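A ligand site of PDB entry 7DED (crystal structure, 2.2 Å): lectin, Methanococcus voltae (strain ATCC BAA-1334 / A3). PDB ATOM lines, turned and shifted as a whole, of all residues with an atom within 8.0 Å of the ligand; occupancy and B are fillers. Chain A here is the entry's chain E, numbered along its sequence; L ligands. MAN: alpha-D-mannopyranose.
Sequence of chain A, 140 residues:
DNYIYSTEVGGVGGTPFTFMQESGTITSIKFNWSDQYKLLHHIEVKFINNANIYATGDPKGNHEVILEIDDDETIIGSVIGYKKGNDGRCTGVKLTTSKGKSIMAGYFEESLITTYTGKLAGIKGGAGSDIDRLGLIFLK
A ring nitrogen (ND1) of His 41 sits at hydrogen-bond distance from the side-chain carboxylate (OD1) of Asp 130 (2.9 Å). OD2 of Asp 130 lies within salt-bridge range of NE of Arg 89 (2.9 Å). OD1 of Asp 132 lies close to N of Gly 14. The side-chain carboxylate of Asp 132 sits at hydrogen-bond distance from the backbone NH of Gly 128. The side-chain carboxylate (OD2) of Asp 132 is in salt-bridge range of the guanidinium group (NH2) of Arg 89 (3.4 Å). The backbone carbonyl oxygen of Asp 132 sits at hydrogen-bond distance from the backbone NH of Gly 11. NH2 of Arg 89 lies within salt-bridge range of OD1 of Asp 87, at 3.2 Å. The backbone carbonyl oxygen (O) of Ser 129 sits at hydrogen-bond distance from a ring nitrogen (ND1) of His 41 (3.1 Å).
An oxygen (O6) of the ligand is in hydrogen-bond range of the backbone NH (N) of Gly 128, 3.1 Å away. O6 of the ligand lies within hydrogen-bond range of OD1 of Asp 132. The backbone carbonyl oxygen (O) of Asp 130 sits at hydrogen-bond distance from an oxygen (O6) of the ligand (3.1 Å). OG of Ser 129 is in hydrogen-bond range of O5 of the ligand. An oxygen (O5) of the ligand is in hydrogen-bond range of the backbone NH of Ser 129, 3.2 Å away. N of Gly 14 lies within hydrogen-bond range of O3 of the ligand. The backbone NH (N) of Asp 130 sits at hydrogen-bond distance from an oxygen (O6) of the ligand (3.2 Å).
Residues that only touch the ligand: Gly 13 (3.7 Å) and Arg 89 (3.9 Å). Seven residues have an atom within 4 Å of the ligand: Gly 13, Gly 14, Arg 89, Gly 128, Ser 129, Asp 130 and Asp 132.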
ATOM      1  N   GLY A  11     -15.260  -9.812  23.865  1.00  0.00           N
ATOM      2  CA  GLY A  11     -16.625  -9.295  24.099  1.00  0.00           C
ATOM      3  C   GLY A  11     -17.229  -9.832  25.372  1.00  0.00           C
ATOM      4  O   GLY A  11     -16.599 -10.682  26.068  1.00  0.00           O
ATOM      5  N   VAL A  12     -18.449  -9.384  25.642  1.00  0.00           N
ATOM      6  CA  VAL A  12     -19.276  -9.771  26.825  1.00  0.00           C
ATOM      7  C   VAL A  12     -20.161 -10.949  26.435  1.00  0.00           C
ATOM      8  O   VAL A  12     -20.738 -11.534  27.370  1.00  0.00           O
ATOM      9  CB  VAL A  12     -20.093  -8.563  27.318  1.00  0.00           C
ATOM     10  CG1 VAL A  12     -19.187  -7.412  27.747  1.00  0.00           C
ATOM     11  CG2 VAL A  12     -21.118  -8.059  26.300  1.00  0.00           C
ATOM     12  N   GLY A  13     -20.209 -11.323  25.130  1.00  0.00           N
ATOM     13  CA  GLY A  13     -21.065 -12.412  24.606  1.00  0.00           C
ATOM     14  C   GLY A  13     -20.683 -13.813  25.099  1.00  0.00           C
ATOM     15  O   GLY A  13     -19.637 -13.976  25.829  1.00  0.00           O
ATOM     16  N   GLY A  14     -21.484 -14.817  24.727  1.00  0.00           N
ATOM     17  CA  GLY A  14     -21.176 -16.241  24.937  1.00  0.00           C
ATOM     18  C   GLY A  14     -21.561 -16.739  26.317  1.00  0.00           C
ATOM     19  O   GLY A  14     -21.851 -15.949  27.190  1.00  0.00           O
ATOM     20  N   THR A  15     -21.523 -18.066  26.487  1.00  0.00           N
ATOM     21  CA  THR A  15     -21.786 -18.752  27.773  1.00  0.00           C
ATOM     22  C   THR A  15     -20.482 -18.756  28.562  1.00  0.00           C
ATOM     23  O   THR A  15     -19.442 -19.149  28.037  1.00  0.00           O
ATOM     24  CB  THR A  15     -22.319 -20.174  27.532  1.00  0.00           C
ATOM     25  N   LEU A  39     -11.548 -15.824  13.249  1.00  0.00           N
ATOM     26  CA  LEU A  39     -11.825 -15.916  14.724  1.00  0.00           C
ATOM     27  C   LEU A  39     -11.311 -17.240  15.285  1.00  0.00           C
ATOM     28  O   LEU A  39     -11.260 -18.201  14.535  1.00  0.00           O
ATOM     29  CB  LEU A  39     -13.335 -15.863  14.975  1.00  0.00           C
ATOM     30  CG  LEU A  39     -14.076 -14.608  14.508  1.00  0.00           C
ATOM     31  CD1 LEU A  39     -15.548 -14.631  14.935  1.00  0.00           C
ATOM     32  CD2 LEU A  39     -13.394 -13.355  15.039  1.00  0.00           C
ATOM     33  N   LEU A  40     -11.048 -17.308  16.588  1.00  0.00           N
ATOM     34  CA  LEU A  40     -11.067 -18.599  17.312  1.00  0.00           C
ATOM     35  C   LEU A  40     -12.526 -19.018  17.501  1.00  0.00           C
ATOM     36  O   LEU A  40     -13.372 -18.149  17.863  1.00  0.00           O
ATOM     37  CB  LEU A  40     -10.387 -18.451  18.678  1.00  0.00           C
ATOM     38  CG  LEU A  40      -8.969 -17.927  18.644  1.00  0.00           C
ATOM     39  CD1 LEU A  40      -8.331 -18.169  19.994  1.00  0.00           C
ATOM     40  CD2 LEU A  40      -8.116 -18.598  17.575  1.00  0.00           C
ATOM     41  N   HIS A  41     -12.806 -20.301  17.292  1.00  0.00           N
ATOM     42  CA  HIS A  41     -14.170 -20.851  17.511  1.00  0.00           C
ATOM     43  C   HIS A  41     -14.229 -21.811  18.705  1.00  0.00           C
ATOM     44  O   HIS A  41     -15.290 -21.910  19.310  1.00  0.00           O
ATOM     45  CB  HIS A  41     -14.657 -21.523  16.219  1.00  0.00           C
ATOM     46  CG  HIS A  41     -14.769 -20.586  15.072  1.00  0.00           C
ATOM     47  ND1 HIS A  41     -15.824 -19.693  14.986  1.00  0.00           N
ATOM     48  CD2 HIS A  41     -13.980 -20.418  13.984  1.00  0.00           C
ATOM     49  CE1 HIS A  41     -15.666 -18.989  13.858  1.00  0.00           C
ATOM     50  NE2 HIS A  41     -14.537 -19.424  13.220  1.00  0.00           N
ATOM     51  N   GLY A  57     -17.040 -23.667  22.881  1.00  0.00           N
ATOM     52  CA  GLY A  57     -17.186 -23.153  21.520  1.00  0.00           C
ATOM     53  C   GLY A  57     -17.587 -24.244  20.546  1.00  0.00           C
ATOM     54  O   GLY A  57     -17.914 -25.326  20.975  1.00  0.00           O
ATOM     55  N   ASP A  58     -17.523 -23.957  19.255  1.00  0.00           N
ATOM     56  CA  ASP A  58     -18.014 -24.835  18.174  1.00  0.00           C
ATOM     57  C   ASP A  58     -16.837 -25.097  17.238  1.00  0.00           C
ATOM     58  O   ASP A  58     -16.321 -24.181  16.622  1.00  0.00           O
ATOM     59  CB  ASP A  58     -19.202 -24.173  17.489  1.00  0.00           C
ATOM     60  CG  ASP A  58     -19.770 -24.909  16.271  1.00  0.00           C
ATOM     61  OD1 ASP A  58     -19.182 -25.937  15.850  1.00  0.00           O
ATOM     62  OD2 ASP A  58     -20.732 -24.373  15.716  1.00  0.00           O
ATOM     63  N   LYS A  60     -15.924 -25.410  14.307  1.00  0.00           N
ATOM     64  CA  LYS A  60     -16.358 -25.243  12.897  1.00  0.00           C
ATOM     65  C   LYS A  60     -15.214 -24.750  12.016  1.00  0.00           C
ATOM     66  O   LYS A  60     -15.392 -24.644  10.835  1.00  0.00           O
ATOM     67  CB  LYS A  60     -17.555 -24.295  12.837  1.00  0.00           C
ATOM     68  CG  LYS A  60     -17.273 -22.826  13.140  1.00  0.00           C
ATOM     69  CD  LYS A  60     -18.392 -21.913  12.758  1.00  0.00           C
ATOM     70  CE  LYS A  60     -19.356 -21.594  13.878  1.00  0.00           C
ATOM     71  NZ  LYS A  60     -20.403 -20.673  13.385  1.00  0.00           N
ATOM     72  N   ASN A  86     -18.076  -4.529  23.218  1.00  0.00           N
ATOM     73  CA  ASN A  86     -19.152  -5.434  23.693  1.00  0.00           C
ATOM     74  C   ASN A  86     -19.261  -6.652  22.762  1.00  0.00           C
ATOM     75  O   ASN A  86     -19.383  -7.759  23.306  1.00  0.00           O
ATOM     76  CB  ASN A  86     -20.477  -4.688  23.867  1.00  0.00           C
ATOM     77  CG  ASN A  86     -20.477  -3.796  25.087  1.00  0.00           C
ATOM     78  OD1 ASN A  86     -19.700  -3.996  26.042  1.00  0.00           O
ATOM     79  ND2 ASN A  86     -21.340  -2.795  25.040  1.00  0.00           N
ATOM     80  N   ASP A  87     -19.219  -6.461  21.439  1.00  0.00           N
ATOM     81  CA  ASP A  87     -19.393  -7.557  20.450  1.00  0.00           C
ATOM     82  C   ASP A  87     -17.976  -8.002  20.010  1.00  0.00           C
ATOM     83  O   ASP A  87     -17.785  -8.450  18.859  1.00  0.00           O
ATOM     84  CB  ASP A  87     -20.370  -7.177  19.324  1.00  0.00           C
ATOM     85  CG  ASP A  87     -20.881  -8.359  18.474  1.00  0.00           C
ATOM     86  OD1 ASP A  87     -21.236  -9.445  19.030  1.00  0.00           O
ATOM     87  OD2 ASP A  87     -20.903  -8.232  17.229  1.00  0.00           O
ATOM     88  N   GLY A  88     -17.007  -7.983  20.926  1.00  0.00           N
ATOM     89  CA  GLY A  88     -15.658  -8.475  20.662  1.00  0.00           C
ATOM     90  C   GLY A  88     -15.558  -9.998  20.637  1.00  0.00           C
ATOM     91  O   GLY A  88     -16.518 -10.679  21.063  1.00  0.00           O
ATOM     92  N   ARG A  89     -14.402 -10.487  20.176  1.00  0.00           N
ATOM     93  CA  ARG A  89     -14.063 -11.901  19.950  1.00  0.00           C
ATOM     94  C   ARG A  89     -12.554 -12.072  20.189  1.00  0.00           C
ATOM     95  O   ARG A  89     -11.851 -11.077  19.960  1.00  0.00           O
ATOM     96  CB  ARG A  89     -14.360 -12.231  18.488  1.00  0.00           C
ATOM     97  CG  ARG A  89     -15.829 -12.091  18.095  1.00  0.00           C
ATOM     98  CD  ARG A  89     -16.690 -13.164  18.749  1.00  0.00           C
ATOM     99  NE  ARG A  89     -18.006 -13.263  18.093  1.00  0.00           N
ATOM    100  CZ  ARG A  89     -19.023 -12.455  18.376  1.00  0.00           C
ATOM    101  NH1 ARG A  89     -20.132 -12.481  17.694  1.00  0.00           N
ATOM    102  NH2 ARG A  89     -18.930 -11.608  19.389  1.00  0.00           N
ATOM    103  N   GLY A 126     -15.815 -16.613  27.736  1.00  0.00           N
ATOM    104  CA  GLY A 126     -17.161 -16.787  27.196  1.00  0.00           C
ATOM    105  C   GLY A 126     -17.073 -17.360  25.787  1.00  0.00           C
ATOM    106  O   GLY A 126     -16.234 -16.891  25.003  1.00  0.00           O
ATOM    107  N   ALA A 127     -17.911 -18.336  25.475  1.00  0.00           N
ATOM    108  CA  ALA A 127     -17.937 -18.950  24.128  1.00  0.00           C
ATOM    109  C   ALA A 127     -19.380 -19.299  23.736  1.00  0.00           C
ATOM    110  O   ALA A 127     -20.190 -19.640  24.651  1.00  0.00           O
ATOM    111  CB  ALA A 127     -17.042 -20.174  24.088  1.00  0.00           C
ATOM    112  N   GLY A 128     -19.654 -19.186  22.430  1.00  0.00           N
ATOM    113  CA  GLY A 128     -20.802 -19.828  21.773  1.00  0.00           C
ATOM    114  C   GLY A 128     -20.369 -20.479  20.467  1.00  0.00           C
ATOM    115  O   GLY A 128     -19.745 -21.541  20.523  1.00  0.00           O
ATOM    116  N   SER A 129     -20.687 -19.849  19.349  1.00  0.00           N
ATOM    117  CA  SER A 129     -20.189 -20.226  18.011  1.00  0.00           C
ATOM    118  C   SER A 129     -18.707 -19.811  17.879  1.00  0.00           C
ATOM    119  O   SER A 129     -17.978 -20.414  17.049  1.00  0.00           O
ATOM    120  CB  SER A 129     -21.036 -19.618  16.934  1.00  0.00           C
ATOM    121  OG  SER A 129     -22.410 -19.813  17.214  1.00  0.00           O
ATOM    122  N   ASP A 130     -18.309 -18.782  18.627  1.00  0.00           N
ATOM    123  CA  ASP A 130     -16.937 -18.237  18.588  1.00  0.00           C
ATOM    124  C   ASP A 130     -16.414 -18.233  20.024  1.00  0.00           C
ATOM    125  O   ASP A 130     -17.249 -18.369  20.972  1.00  0.00           O
ATOM    126  CB  ASP A 130     -16.920 -16.844  17.978  1.00  0.00           C
ATOM    127  CG  ASP A 130     -17.740 -16.752  16.709  1.00  0.00           C
ATOM    128  OD1 ASP A 130     -17.757 -17.776  15.970  1.00  0.00           O
ATOM    129  OD2 ASP A 130     -18.409 -15.684  16.480  1.00  0.00           O
ATOM    130  N   ILE A 131     -15.105 -18.036  20.199  1.00  0.00           N
ATOM    131  CA  ILE A 131     -14.541 -17.655  21.521  1.00  0.00           C
ATOM    132  C   ILE A 131     -14.712 -16.141  21.679  1.00  0.00           C
ATOM    133  O   ILE A 131     -14.002 -15.379  20.993  1.00  0.00           O
ATOM    134  CB  ILE A 131     -13.082 -18.075  21.644  1.00  0.00           C
ATOM    135  CG1 ILE A 131     -12.871 -19.546  21.275  1.00  0.00           C
ATOM    136  CG2 ILE A 131     -12.609 -17.750  23.059  1.00  0.00           C
ATOM    137  CD1 ILE A 131     -13.568 -20.501  22.225  1.00  0.00           C
ATOM    138  N   ASP A 132     -15.662 -15.736  22.523  1.00  0.00           N
ATOM    139  CA  ASP A 132     -16.005 -14.319  22.740  1.00  0.00           C
ATOM    140  C   ASP A 132     -14.881 -13.659  23.529  1.00  0.00           C
ATOM    141  O   ASP A 132     -14.524 -12.510  23.257  1.00  0.00           O
ATOM    142  CB  ASP A 132     -17.343 -14.177  23.470  1.00  0.00           C
ATOM    143  CG  ASP A 132     -18.550 -14.628  22.649  1.00  0.00           C
ATOM    144  OD1 ASP A 132     -18.836 -15.843  22.684  1.00  0.00           O
ATOM    145  OD2 ASP A 132     -19.173 -13.771  21.975  1.00  0.00           O
ATOM    146  N   ARG A 133     -14.310 -14.389  24.464  1.00  0.00           N
ATOM    147  CA  ARG A 133     -13.547 -13.795  25.581  1.00  0.00           C
ATOM    148  C   ARG A 133     -12.636 -14.889  26.080  1.00  0.00           C
ATOM    149  O   ARG A 133     -13.157 -15.994  26.235  1.00  0.00           O
ATOM    150  CB  ARG A 133     -14.564 -13.315  26.617  1.00  0.00           C
ATOM    151  CG  ARG A 133     -13.977 -12.654  27.860  1.00  0.00           C
ATOM    152  CD  ARG A 133     -14.999 -11.948  28.754  1.00  0.00           C
ATOM    153  NE  ARG A 133     -16.344 -12.344  28.348  1.00  0.00           N
ATOM    154  CZ  ARG A 133     -17.081 -13.299  28.914  1.00  0.00           C
ATOM    155  NH1 ARG A 133     -16.625 -13.918  29.995  1.00  0.00           N
ATOM    156  NH2 ARG A 133     -18.267 -13.576  28.428  1.00  0.00           N
HETATM  157  C1  MAN L   1     -23.885 -17.214  19.541  1.00  0.00           C
HETATM  158  C2  MAN L   1     -24.335 -16.871  20.961  1.00  0.00           C
HETATM  159  C3  MAN L   1     -23.744 -15.539  21.422  1.00  0.00           C
HETATM  160  C4  MAN L   1     -22.240 -15.502  21.168  1.00  0.00           C
HETATM  161  C5  MAN L   1     -21.912 -15.929  19.742  1.00  0.00           C
HETATM  162  C6  MAN L   1     -20.407 -15.953  19.514  1.00  0.00           C
HETATM  163  O1  MAN L   1     -24.393 -16.233  18.636  1.00  0.00           O
HETATM  164  O2  MAN L   1     -23.926 -17.904  21.860  1.00  0.00           O
HETATM  165  O3  MAN L   1     -23.999 -15.352  22.816  1.00  0.00           O
HETATM  166  O4  MAN L   1     -21.741 -14.179  21.404  1.00  0.00           O
HETATM  167  O5  MAN L   1     -22.455 -17.219  19.491  1.00  0.00           O
HETATM  168  O6  MAN L   1     -19.778 -16.712  20.561  1.00  0.00           O
